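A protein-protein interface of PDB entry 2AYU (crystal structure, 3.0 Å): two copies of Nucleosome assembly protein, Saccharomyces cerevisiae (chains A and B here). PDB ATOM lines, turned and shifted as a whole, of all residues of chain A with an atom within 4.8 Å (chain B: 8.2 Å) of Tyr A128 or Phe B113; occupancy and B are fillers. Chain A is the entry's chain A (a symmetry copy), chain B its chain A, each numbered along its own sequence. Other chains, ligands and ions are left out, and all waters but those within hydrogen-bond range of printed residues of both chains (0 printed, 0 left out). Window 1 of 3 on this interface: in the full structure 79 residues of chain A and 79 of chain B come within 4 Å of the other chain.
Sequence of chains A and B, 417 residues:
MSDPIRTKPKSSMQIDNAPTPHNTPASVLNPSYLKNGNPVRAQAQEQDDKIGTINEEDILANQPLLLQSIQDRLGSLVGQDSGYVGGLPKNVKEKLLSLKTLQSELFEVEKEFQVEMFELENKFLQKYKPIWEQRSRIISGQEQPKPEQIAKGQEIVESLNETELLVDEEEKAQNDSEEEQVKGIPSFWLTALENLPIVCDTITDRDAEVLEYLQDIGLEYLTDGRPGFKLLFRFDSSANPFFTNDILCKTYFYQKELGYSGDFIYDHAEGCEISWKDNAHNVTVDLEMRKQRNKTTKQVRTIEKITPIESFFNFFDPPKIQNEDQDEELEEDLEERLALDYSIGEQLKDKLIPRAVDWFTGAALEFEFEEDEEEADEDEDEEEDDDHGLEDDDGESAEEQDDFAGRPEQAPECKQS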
ATOM      1  N   LEU A 120      14.717 -19.462  28.350  1.00  0.00           N
ATOM      2  CA  LEU A 120      15.873 -20.087  27.715  1.00  0.00           C
ATOM      3  C   LEU A 120      16.199 -19.385  26.404  1.00  0.00           C
ATOM      4  O   LEU A 120      17.369 -19.234  26.042  1.00  0.00           O
ATOM      5  CB  LEU A 120      15.599 -21.570  27.457  1.00  0.00           C
ATOM      6  CG  LEU A 120      16.790 -22.407  26.967  1.00  0.00           C
ATOM      7  CD1 LEU A 120      16.425 -23.883  26.990  1.00  0.00           C
ATOM      8  CD2 LEU A 120      17.188 -22.010  25.567  1.00  0.00           C
ATOM      9  N   GLU A 121      15.156 -18.962  25.696  1.00  0.00           N
ATOM     10  CA  GLU A 121      15.306 -18.269  24.423  1.00  0.00           C
ATOM     11  C   GLU A 121      15.934 -16.906  24.625  1.00  0.00           C
ATOM     12  O   GLU A 121      16.892 -16.538  23.944  1.00  0.00           O
ATOM     13  CB  GLU A 121      13.944 -18.109  23.747  1.00  0.00           C
ATOM     14  CG  GLU A 121      13.473 -19.350  23.019  1.00  0.00           C
ATOM     15  CD  GLU A 121      11.975 -19.381  22.846  1.00  0.00           C
ATOM     16  OE1 GLU A 121      11.401 -18.355  22.427  1.00  0.00           O
ATOM     17  OE2 GLU A 121      11.369 -20.434  23.128  1.00  0.00           O
ATOM     18  N   PHE A 124      19.656 -16.968  25.128  1.00  0.00           N
ATOM     19  CA  PHE A 124      20.522 -17.012  23.971  1.00  0.00           C
ATOM     20  C   PHE A 124      20.417 -15.798  23.087  1.00  0.00           C
ATOM     21  O   PHE A 124      21.347 -15.493  22.335  1.00  0.00           O
ATOM     22  CB  PHE A 124      20.267 -18.283  23.207  1.00  0.00           C
ATOM     23  CG  PHE A 124      20.898 -19.458  23.845  1.00  0.00           C
ATOM     24  CD1 PHE A 124      21.979 -20.096  23.239  1.00  0.00           C
ATOM     25  CD2 PHE A 124      20.464 -19.897  25.098  1.00  0.00           C
ATOM     26  CE1 PHE A 124      22.619 -21.161  23.880  1.00  0.00           C
ATOM     27  CE2 PHE A 124      21.101 -20.960  25.745  1.00  0.00           C
ATOM     28  CZ  PHE A 124      22.177 -21.591  25.135  1.00  0.00           C
ATOM     29  N   LEU A 125      19.297 -15.088  23.186  1.00  0.00           N
ATOM     30  CA  LEU A 125      19.150 -13.888  22.391  1.00  0.00           C
ATOM     31  C   LEU A 125      20.340 -13.052  22.801  1.00  0.00           C
ATOM     32  O   LEU A 125      20.972 -12.383  21.983  1.00  0.00           O
ATOM     33  CB  LEU A 125      17.863 -13.139  22.732  1.00  0.00           C
ATOM     34  CG  LEU A 125      17.836 -11.725  22.122  1.00  0.00           C
ATOM     35  CD1 LEU A 125      17.864 -11.801  20.606  1.00  0.00           C
ATOM     36  CD2 LEU A 125      16.597 -10.985  22.598  1.00  0.00           C
ATOM     37  N   GLN A 126      20.639 -13.123  24.093  1.00  0.00           N
ATOM     38  CA  GLN A 126      21.743 -12.392  24.680  1.00  0.00           C
ATOM     39  C   GLN A 126      23.056 -12.790  24.039  1.00  0.00           C
ATOM     40  O   GLN A 126      23.869 -11.936  23.683  1.00  0.00           O
ATOM     41  CB  GLN A 126      21.796 -12.659  26.178  1.00  0.00           C
ATOM     42  CG  GLN A 126      20.493 -12.351  26.873  1.00  0.00           C
ATOM     43  CD  GLN A 126      19.824 -11.114  26.308  1.00  0.00           C
ATOM     44  OE1 GLN A 126      20.491 -10.146  25.945  1.00  0.00           O
ATOM     45  NE2 GLN A 126      18.495 -11.138  26.236  1.00  0.00           N
ATOM     46  N   LYS A 127      23.260 -14.090  23.886  1.00  0.00           N
ATOM     47  CA  LYS A 127      24.485 -14.588  23.288  1.00  0.00           C
ATOM     48  C   LYS A 127      24.607 -14.226  21.801  1.00  0.00           C
ATOM     49  O   LYS A 127      25.717 -14.218  21.249  1.00  0.00           O
ATOM     50  CB  LYS A 127      24.562 -16.100  23.497  1.00  0.00           C
ATOM     51  CG  LYS A 127      24.393 -16.472  24.954  1.00  0.00           C
ATOM     52  CD  LYS A 127      24.506 -17.961  25.207  1.00  0.00           C
ATOM     53  CE  LYS A 127      24.191 -18.278  26.673  1.00  0.00           C
ATOM     54  NZ  LYS A 127      24.388 -19.715  27.069  1.00  0.00           N
ATOM     55  N   TYR A 128      23.479 -13.917  21.157  1.00  0.00           N
ATOM     56  CA  TYR A 128      23.507 -13.552  19.740  1.00  0.00           C
ATOM     57  C   TYR A 128      23.799 -12.066  19.583  1.00  0.00           C
ATOM     58  O   TYR A 128      24.657 -11.687  18.781  1.00  0.00           O
ATOM     59  CB  TYR A 128      22.169 -13.861  19.037  1.00  0.00           C
ATOM     60  CG  TYR A 128      21.698 -15.303  19.094  1.00  0.00           C
ATOM     61  CD1 TYR A 128      22.587 -16.362  18.909  1.00  0.00           C
ATOM     62  CD2 TYR A 128      20.357 -15.610  19.359  1.00  0.00           C
ATOM     63  CE1 TYR A 128      22.155 -17.704  19.003  1.00  0.00           C
ATOM     64  CE2 TYR A 128      19.913 -16.944  19.451  1.00  0.00           C
ATOM     65  CZ  TYR A 128      20.820 -17.983  19.280  1.00  0.00           C
ATOM     66  OH  TYR A 128      20.415 -19.287  19.445  1.00  0.00           O
ATOM     67  N   LYS A 129      23.086 -11.241  20.363  1.00  0.00           N
ATOM     68  CA  LYS A 129      23.211  -9.774  20.324  1.00  0.00           C
ATOM     69  C   LYS A 129      24.603  -9.282  19.973  1.00  0.00           C
ATOM     70  O   LYS A 129      24.764  -8.488  19.051  1.00  0.00           O
ATOM     71  CB  LYS A 129      22.765  -9.130  21.651  1.00  0.00           C
ATOM     72  CG  LYS A 129      21.261  -9.233  21.930  1.00  0.00           C
ATOM     73  CD  LYS A 129      20.714  -7.989  22.657  1.00  0.00           C
ATOM     74  CE  LYS A 129      19.179  -8.041  22.791  1.00  0.00           C
ATOM     75  NZ  LYS A 129      18.564  -6.703  23.057  1.00  0.00           N
ATOM     76  N   PRO A 130      25.633  -9.753  20.699  1.00  0.00           N
ATOM     77  CA  PRO A 130      27.021  -9.349  20.446  1.00  0.00           C
ATOM     78  C   PRO A 130      27.379  -9.523  18.979  1.00  0.00           C
ATOM     79  O   PRO A 130      27.841  -8.581  18.319  1.00  0.00           O
ATOM     80  CB  PRO A 130      27.815 -10.294  21.329  1.00  0.00           C
ATOM     81  CG  PRO A 130      26.879 -10.547  22.466  1.00  0.00           C
ATOM     82  CD  PRO A 130      25.576 -10.760  21.773  1.00  0.00           C
ATOM     83  N   ILE A 131      27.152 -10.740  18.485  1.00  0.00           N
ATOM     84  CA  ILE A 131      27.437 -11.066  17.100  1.00  0.00           C
ATOM     85  C   ILE A 131      26.637 -10.150  16.180  1.00  0.00           C
ATOM     86  O   ILE A 131      27.209  -9.466  15.327  1.00  0.00           O
ATOM     87  CB  ILE A 131      27.060 -12.515  16.745  1.00  0.00           C
ATOM     88  CG1 ILE A 131      27.286 -13.458  17.929  1.00  0.00           C
ATOM     89  CG2 ILE A 131      27.922 -12.982  15.596  1.00  0.00           C
ATOM     90  CD1 ILE A 131      26.868 -14.934  17.646  1.00  0.00           C
ATOM     91  N   TRP A 132      25.318 -10.128  16.345  1.00  0.00           N
ATOM     92  CA  TRP A 132      24.503  -9.283  15.488  1.00  0.00           C
ATOM     93  C   TRP A 132      24.950  -7.821  15.496  1.00  0.00           C
ATOM     94  O   TRP A 132      24.879  -7.145  14.464  1.00  0.00           O
ATOM     95  CB  TRP A 132      23.020  -9.392  15.862  1.00  0.00           C
ATOM     96  CG  TRP A 132      22.429 -10.731  15.526  1.00  0.00           C
ATOM     97  CD1 TRP A 132      22.844 -11.576  14.544  1.00  0.00           C
ATOM     98  CD2 TRP A 132      21.317 -11.377  16.164  1.00  0.00           C
ATOM     99  NE1 TRP A 132      22.070 -12.710  14.529  1.00  0.00           N
ATOM    100  CE2 TRP A 132      21.124 -12.616  15.513  1.00  0.00           C
ATOM    101  CE3 TRP A 132      20.464 -11.031  17.221  1.00  0.00           C
ATOM    102  CZ2 TRP A 132      20.114 -13.513  15.882  1.00  0.00           C
ATOM    103  CZ3 TRP A 132      19.452 -11.929  17.591  1.00  0.00           C
ATOM    104  CH2 TRP A 132      19.291 -13.153  16.920  1.00  0.00           C
ATOM    105  N   LEU B 102      30.711 -14.373  10.535  1.00  0.00           N
ATOM    106  CA  LEU B 102      29.933 -14.070  11.719  1.00  0.00           C
ATOM    107  C   LEU B 102      28.758 -15.030  11.798  1.00  0.00           C
ATOM    108  O   LEU B 102      28.325 -15.391  12.890  1.00  0.00           O
ATOM    109  CB  LEU B 102      29.432 -12.628  11.662  1.00  0.00           C
ATOM    110  CG  LEU B 102      30.114 -11.623  12.591  1.00  0.00           C
ATOM    111  CD1 LEU B 102      31.607 -11.851  12.635  1.00  0.00           C
ATOM    112  CD2 LEU B 102      29.814 -10.230  12.098  1.00  0.00           C
ATOM    113  N   GLU B 105      29.556 -18.277  13.424  1.00  0.00           N
ATOM    114  CA  GLU B 105      29.762 -18.074  14.858  1.00  0.00           C
ATOM    115  C   GLU B 105      28.405 -18.264  15.519  1.00  0.00           C
ATOM    116  O   GLU B 105      28.272 -19.034  16.476  1.00  0.00           O
ATOM    117  CB  GLU B 105      30.283 -16.667  15.122  1.00  0.00           C
ATOM    118  CG  GLU B 105      31.572 -16.366  14.397  1.00  0.00           C
ATOM    119  CD  GLU B 105      32.236 -15.113  14.912  1.00  0.00           C
ATOM    120  OE1 GLU B 105      31.700 -14.014  14.670  1.00  0.00           O
ATOM    121  OE2 GLU B 105      33.292 -15.227  15.569  1.00  0.00           O
ATOM    122  N   LEU B 106      27.410 -17.547  14.991  1.00  0.00           N
ATOM    123  CA  LEU B 106      26.026 -17.642  15.446  1.00  0.00           C
ATOM    124  C   LEU B 106      25.753 -19.138  15.521  1.00  0.00           C
ATOM    125  O   LEU B 106      25.384 -19.676  16.564  1.00  0.00           O
ATOM    126  CB  LEU B 106      25.097 -17.040  14.399  1.00  0.00           C
ATOM    127  CG  LEU B 106      24.258 -15.790  14.655  1.00  0.00           C
ATOM    128  CD1 LEU B 106      23.816 -15.217  13.287  1.00  0.00           C
ATOM    129  CD2 LEU B 106      23.056 -16.115  15.538  1.00  0.00           C
ATOM    130  N   PHE B 107      25.955 -19.804  14.390  1.00  0.00           N
ATOM    131  CA  PHE B 107      25.750 -21.238  14.286  1.00  0.00           C
ATOM    132  C   PHE B 107      26.281 -22.047  15.472  1.00  0.00           C
ATOM    133  O   PHE B 107      25.613 -22.955  15.976  1.00  0.00           O
ATOM    134  CB  PHE B 107      26.374 -21.743  12.988  1.00  0.00           C
ATOM    135  CG  PHE B 107      25.428 -21.726  11.838  1.00  0.00           C
ATOM    136  CD1 PHE B 107      24.981 -20.524  11.315  1.00  0.00           C
ATOM    137  CD2 PHE B 107      24.916 -22.922  11.328  1.00  0.00           C
ATOM    138  CE1 PHE B 107      24.035 -20.503  10.309  1.00  0.00           C
ATOM    139  CE2 PHE B 107      23.962 -22.924  10.320  1.00  0.00           C
ATOM    140  CZ  PHE B 107      23.519 -21.704   9.809  1.00  0.00           C
ATOM    141  N   GLU B 108      27.479 -21.719  15.926  1.00  0.00           N
ATOM    142  CA  GLU B 108      28.052 -22.449  17.036  1.00  0.00           C
ATOM    143  C   GLU B 108      27.222 -22.236  18.314  1.00  0.00           C
ATOM    144  O   GLU B 108      27.098 -23.138  19.153  1.00  0.00           O
ATOM    145  CB  GLU B 108      29.494 -22.006  17.230  1.00  0.00           C
ATOM    146  CG  GLU B 108      30.251 -22.807  18.252  1.00  0.00           C
ATOM    147  CD  GLU B 108      31.662 -22.299  18.419  1.00  0.00           C
ATOM    148  OE1 GLU B 108      32.467 -22.484  17.478  1.00  0.00           O
ATOM    149  OE2 GLU B 108      31.962 -21.702  19.480  1.00  0.00           O
ATOM    150  N   VAL B 109      26.647 -21.045  18.451  1.00  0.00           N
ATOM    151  CA  VAL B 109      25.817 -20.713  19.617  1.00  0.00           C
ATOM    152  C   VAL B 109      24.486 -21.472  19.521  1.00  0.00           C
ATOM    153  O   VAL B 109      24.025 -22.126  20.472  1.00  0.00           O
ATOM    154  CB  VAL B 109      25.442 -19.199  19.656  1.00  0.00           C
ATOM    155  CG1 VAL B 109      24.896 -18.840  21.031  1.00  0.00           C
ATOM    156  CG2 VAL B 109      26.615 -18.330  19.256  1.00  0.00           C
ATOM    157  N   GLU B 110      23.875 -21.341  18.346  1.00  0.00           N
ATOM    158  CA  GLU B 110      22.599 -21.957  18.037  1.00  0.00           C
ATOM    159  C   GLU B 110      22.620 -23.457  18.282  1.00  0.00           C
ATOM    160  O   GLU B 110      21.564 -24.078  18.470  1.00  0.00           O
ATOM    161  CB  GLU B 110      22.226 -21.640  16.588  1.00  0.00           C
ATOM    162  CG  GLU B 110      22.364 -20.145  16.271  1.00  0.00           C
ATOM    163  CD  GLU B 110      21.650 -19.724  14.992  1.00  0.00           C
ATOM    164  OE1 GLU B 110      21.790 -20.436  13.962  1.00  0.00           O
ATOM    165  OE2 GLU B 110      20.959 -18.674  15.026  1.00  0.00           O
ATOM    166  N   LYS B 111      23.816 -24.045  18.275  1.00  0.00           N
ATOM    167  CA  LYS B 111      23.906 -25.462  18.540  1.00  0.00           C
ATOM    168  C   LYS B 111      23.718 -25.665  20.035  1.00  0.00           C
ATOM    169  O   LYS B 111      22.940 -26.530  20.466  1.00  0.00           O
ATOM    170  CB  LYS B 111      25.239 -26.055  18.091  1.00  0.00           C
ATOM    171  CG  LYS B 111      25.209 -27.555  18.322  1.00  0.00           C
ATOM    172  CD  LYS B 111      26.060 -28.379  17.382  1.00  0.00           C
ATOM    173  CE  LYS B 111      25.627 -29.851  17.474  1.00  0.00           C
ATOM    174  NZ  LYS B 111      26.665 -30.843  17.036  1.00  0.00           N
ATOM    175  N   GLU B 112      24.415 -24.857  20.832  1.00  0.00           N
ATOM    176  CA  GLU B 112      24.287 -24.969  22.282  1.00  0.00           C
ATOM    177  C   GLU B 112      22.826 -24.753  22.663  1.00  0.00           C
ATOM    178  O   GLU B 112      22.255 -25.478  23.484  1.00  0.00           O
ATOM    179  CB  GLU B 112      25.175 -23.943  22.993  1.00  0.00           C
ATOM    180  CG  GLU B 112      25.044 -23.971  24.518  1.00  0.00           C
ATOM    181  CD  GLU B 112      25.101 -25.386  25.101  1.00  0.00           C
ATOM    182  OE1 GLU B 112      26.092 -26.108  24.852  1.00  0.00           O
ATOM    183  OE2 GLU B 112      24.151 -25.776  25.817  1.00  0.00           O
ATOM    184  N   PHE B 113      22.222 -23.746  22.052  1.00  0.00           N
ATOM    185  CA  PHE B 113      20.828 -23.455  22.315  1.00  0.00           C
ATOM    186  C   PHE B 113      20.006 -24.731  22.200  1.00  0.00           C
ATOM    187  O   PHE B 113      19.316 -25.130  23.133  1.00  0.00           O
ATOM    188  CB  PHE B 113      20.287 -22.456  21.303  1.00  0.00           C
ATOM    189  CG  PHE B 113      18.821 -22.239  21.433  1.00  0.00           C
ATOM    190  CD1 PHE B 113      18.322 -21.298  22.320  1.00  0.00           C
ATOM    191  CD2 PHE B 113      17.932 -23.024  20.721  1.00  0.00           C
ATOM    192  CE1 PHE B 113      16.960 -21.147  22.492  1.00  0.00           C
ATOM    193  CE2 PHE B 113      16.571 -22.877  20.890  1.00  0.00           C
ATOM    194  CZ  PHE B 113      16.086 -21.937  21.776  1.00  0.00           C
ATOM    195  N   GLN B 114      20.080 -25.353  21.030  1.00  0.00           N
ATOM    196  CA  GLN B 114      19.342 -26.577  20.767  1.00  0.00           C
ATOM    197  C   GLN B 114      19.574 -27.611  21.835  1.00  0.00           C
ATOM    198  O   GLN B 114      18.674 -28.373  22.178  1.00  0.00           O
ATOM    199  CB  GLN B 114      19.726 -27.155  19.404  1.00  0.00           C
ATOM    200  CG  GLN B 114      18.799 -26.718  18.287  1.00  0.00           C
ATOM    201  CD  GLN B 114      17.376 -27.214  18.489  1.00  0.00           C
ATOM    202  OE1 GLN B 114      16.683 -26.835  19.444  1.00  0.00           O
ATOM    203  NE2 GLN B 114      16.933 -28.076  17.586  1.00  0.00           N
ATOM    204  N   VAL B 115      20.787 -27.630  22.363  1.00  0.00           N
ATOM    205  CA  VAL B 115      21.127 -28.586  23.400  1.00  0.00           C
ATOM    206  C   VAL B 115      20.380 -28.345  24.710  1.00  0.00           C
ATOM    207  O   VAL B 115      19.753 -29.260  25.259  1.00  0.00           O
ATOM    208  CB  VAL B 115      22.611 -28.554  23.660  1.00  0.00           C
ATOM    209  CG1 VAL B 115      22.971 -29.574  24.732  1.00  0.00           C
ATOM    210  CG2 VAL B 115      23.345 -28.809  22.356  1.00  0.00           C
ATOM    211  N   GLU B 116      20.443 -27.117  25.211  1.00  0.00           N
ATOM    212  CA  GLU B 116      19.760 -26.786  26.452  1.00  0.00           C
ATOM    213  C   GLU B 116      18.246 -26.916  26.317  1.00  0.00           C
ATOM    214  O   GLU B 116      17.528 -27.101  27.309  1.00  0.00           O
ATOM    215  CB  GLU B 116      20.154 -25.379  26.891  1.00  0.00           C
ATOM    216  CG  GLU B 116      21.609 -25.297  27.327  1.00  0.00           C
ATOM    217  CD  GLU B 116      21.986 -23.922  27.802  1.00  0.00           C
ATOM    218  OE1 GLU B 116      21.139 -23.297  28.481  1.00  0.00           O
ATOM    219  OE2 GLU B 116      23.121 -23.475  27.507  1.00  0.00           O
ATOM    220  N   MET B 117      17.784 -26.832  25.072  1.00  0.00           N
ATOM    221  CA  MET B 117      16.370 -26.957  24.736  1.00  0.00           C
ATOM    222  C   MET B 117      15.966 -28.421  24.809  1.00  0.00           C
ATOM    223  O   MET B 117      14.986 -28.781  25.451  1.00  0.00           O
ATOM    224  CB  MET B 117      16.118 -26.450  23.311  1.00  0.00           C
ATOM    225  CG  MET B 117      14.638 -26.353  22.915  1.00  0.00           C
ATOM    226  SD  MET B 117      13.738 -25.133  23.926  1.00  0.00           S
ATOM    227  CE  MET B 117      14.795 -23.607  23.716  1.00  0.00           C
ATOM    228  N   PHE B 118      16.731 -29.259  24.128  1.00  0.00           N
ATOM    229  CA  PHE B 118      16.450 -30.678  24.104  1.00  0.00           C
ATOM    230  C   PHE B 118      16.390 -31.169  25.533  1.00  0.00           C
ATOM    231  O   PHE B 118      15.571 -32.030  25.878  1.00  0.00           O
ATOM    232  CB  PHE B 118      17.547 -31.415  23.363  1.00  0.00           C
ATOM    233  CG  PHE B 118      17.283 -32.862  23.220  1.00  0.00           C
ATOM    234  CD1 PHE B 118      16.239 -33.306  22.428  1.00  0.00           C
ATOM    235  CD2 PHE B 118      18.081 -33.793  23.874  1.00  0.00           C
ATOM    236  CE1 PHE B 118      15.992 -34.671  22.280  1.00  0.00           C
ATOM    237  CE2 PHE B 118      17.846 -35.161  23.736  1.00  0.00           C
ATOM    238  CZ  PHE B 118      16.800 -35.601  22.935  1.00  0.00           C
ATOM    239  N   GLU B 119      17.278 -30.616  26.357  1.00  0.00           N
ATOM    240  CA  GLU B 119      17.352 -30.963  27.772  1.00  0.00           C
ATOM    241  C   GLU B 119      16.090 -30.492  28.459  1.00  0.00           C
ATOM    242  O   GLU B 119      15.363 -31.297  29.048  1.00  0.00           O
ATOM    243  CB  GLU B 119      18.545 -30.282  28.414  1.00  0.00           C
ATOM    244  CG  GLU B 119      19.865 -30.922  28.105  1.00  0.00           C
ATOM    245  CD  GLU B 119      20.999 -29.936  28.271  1.00  0.00           C
ATOM    246  OE1 GLU B 119      20.966 -29.150  29.251  1.00  0.00           O
ATOM    247  OE2 GLU B 119      21.925 -29.948  27.429  1.00  0.00           O
ATOM    248  N   LEU B 120      15.843 -29.181  28.370  1.00  0.00           N
ATOM    249  CA  LEU B 120      14.665 -28.559  28.964  1.00  0.00           C
ATOM    250  C   LEU B 120      13.418 -29.370  28.639  1.00  0.00           C
ATOM    251  O   LEU B 120      12.509 -29.490  29.464  1.00  0.00           O
ATOM    252  CB  LEU B 120      14.503 -27.127  28.447  1.00  0.00           C
ATOM    253  CG  LEU B 120      13.417 -26.278  29.125  1.00  0.00           C
ATOM    254  CD1 LEU B 120      13.542 -24.830  28.675  1.00  0.00           C
ATOM    255  CD2 LEU B 120      12.040 -26.791  28.784  1.00  0.00           C
ATOM    256  N   GLU B 121      13.383 -29.922  27.430  1.00  0.00           N
ATOM    257  CA  GLU B 121      12.260 -30.731  26.973  1.00  0.00           C
ATOM    258  C   GLU B 121      12.183 -32.029  27.750  1.00  0.00           C
ATOM    259  O   GLU B 121      11.125 -32.408  28.254  1.00  0.00           O
ATOM    260  CB  GLU B 121      12.403 -31.037  25.482  1.00  0.00           C
ATOM    261  CG  GLU B 121      11.958 -29.905  24.580  1.00  0.00           C
ATOM    262  CD  GLU B 121      12.589 -29.978  23.212  1.00  0.00           C
ATOM    263  OE1 GLU B 121      12.590 -31.072  22.612  1.00  0.00           O
ATOM    264  OE2 GLU B 121      13.085 -28.937  22.735  1.00  0.00           O
ATOM    265  N   LEU B 258      23.084 -29.362  12.410  1.00  0.00           N
ATOM    266  CA  LEU B 258      21.771 -28.755  12.567  1.00  0.00           C
ATOM    267  C   LEU B 258      21.264 -28.200  11.246  1.00  0.00           C
ATOM    268  O   LEU B 258      22.040 -27.968  10.322  1.00  0.00           O
ATOM    269  CB  LEU B 258      21.849 -27.628  13.592  1.00  0.00           C
ATOM    270  CG  LEU B 258      20.850 -27.720  14.732  1.00  0.00           C
ATOM    271  CD1 LEU B 258      21.012 -29.059  15.426  1.00  0.00           C
ATOM    272  CD2 LEU B 258      21.085 -26.573  15.693  1.00  0.00           C
ATOM    273  N   GLY B 262      17.742 -24.113  11.716  1.00  0.00           N
ATOM    274  CA  GLY B 262      18.236 -23.977  13.076  1.00  0.00           C
ATOM    275  C   GLY B 262      17.909 -25.109  14.034  1.00  0.00           C
ATOM    276  O   GLY B 262      18.355 -25.095  15.186  1.00  0.00           O
ATOM    277  N   ASP B 263      17.134 -26.086  13.577  1.00  0.00           N
ATOM    278  CA  ASP B 263      16.767 -27.208  14.432  1.00  0.00           C
ATOM    279  C   ASP B 263      17.217 -28.558  13.896  1.00  0.00           C
ATOM    280  O   ASP B 263      17.688 -28.671  12.754  1.00  0.00           O
ATOM    281  CB  ASP B 263      15.254 -27.224  14.684  1.00  0.00           C
ATOM    282  CG  ASP B 263      14.477 -26.565  13.568  1.00  0.00           C
ATOM    283  OD1 ASP B 263      14.755 -26.891  12.391  1.00  0.00           O
ATOM    284  OD2 ASP B 263      13.591 -25.727  13.869  1.00  0.00           O
ATOM    285  N   PHE B 264      17.060 -29.573  14.747  1.00  0.00           N
ATOM    286  CA  PHE B 264      17.447 -30.949  14.451  1.00  0.00           C
ATOM    287  C   PHE B 264      16.957 -31.470  13.099  1.00  0.00           C
ATOM    288  O   PHE B 264      15.921 -31.045  12.580  1.00  0.00           O
ATOM    289  CB  PHE B 264      16.974 -31.863  15.593  1.00  0.00           C
ATOM    290  CG  PHE B 264      17.727 -31.653  16.891  1.00  0.00           C
ATOM    291  CD1 PHE B 264      17.160 -32.015  18.111  1.00  0.00           C
ATOM    292  CD2 PHE B 264      19.016 -31.100  16.894  1.00  0.00           C
ATOM    293  CE1 PHE B 264      17.865 -31.826  19.317  1.00  0.00           C
ATOM    294  CE2 PHE B 264      19.729 -30.906  18.100  1.00  0.00           C
ATOM    295  CZ  PHE B 264      19.151 -31.270  19.307  1.00  0.00           C
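Leu A120 touches its own counterpart, Leu B120.
Among the printed residues, merely in contact across the chains: Phe A124 with Glu B116 (3.2 Å), Phe A124 with Phe B113 (3.2 Å), Leu A120 with Phe B113 (3.2 Å), Trp A132 with Leu B106 (3.3 Å), Tyr A128 with Leu B106 (3.4 Å), Leu A120 with Glu B116 (3.4 Å), Leu A120 with Met B117 (3.4 Å), Leu A120 with Leu B120 (3.5 Å), Ile A131 with Leu B106 (3.6 Å), Tyr A128 with Val B109 (3.6 Å), Ile A131 with Leu B102 (3.6 Å), Tyr A128 with Glu B110 (3.7 Å), Tyr A128 with Phe B113 (3.7 Å), Lys A127 with Val B109 (3.7 Å), Phe A124 with Glu B112 (3.8 Å), Ile A131 with Val B109 (3.8 Å), Phe A124 with Val B109 (3.8 Å) and Glu A121 with Phe B113 (3.8 Å).
Printed residues of chain B within 4 Å of Phe A124: Val B109 (3.8 Å), Glu B112 (3.8 Å), Phe B113 (3.2 Å) and Glu B116 (3.2 Å). Tyr A128 touches just these residues of chain B: Leu B106 (3.4 Å), Val B109 (3.6 Å), Glu B110 (3.7 Å) and Phe B113 (3.7 Å). Of the printed residues of chain A, Leu B102 touches Ile A131 (3.6 Å). Phe B107 touches none of the printed residues of chain A. Of chain A, only Leu A120, Glu A121, Phe A124 and Tyr A128 come within 4 Å of Phe B113. Of the printed residues of chain A, Glu B116 touches Leu A120 (3.4 Å), Phe A124 (3.2 Å) and Lys A127 (3.99 Å). Of the printed residues of chain A, Leu B120 touches Leu A120 (3.5 Å). The nearest printed residue of chain A that does not touch Phe B113 is Leu A125 (6.3 Å).
NZ of Lys A127 lies within salt-bridge range of OE2 of Glu B116.
Hydrophobic or aromatic side chains of chain B within 4 Å of the printed part of chain A: Leu B102, Leu B106, Val B109, Phe B113, Met B117 and Leu B120. Of the 11 printed residues of chain A, 7 touch a printed residue of chain B. Printed residues of chain A that touch a printed residue of chain B: Leu A120, Glu A121, Phe A124, Lys A127, Tyr A128, Ile A131 and Trp A132. Among the printed residues, Asp or Glu carboxylates within 4 Å of a Lys or Arg side-chain nitrogen of the other chain: Lys A127 with Glu B116 (3.99 Å).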
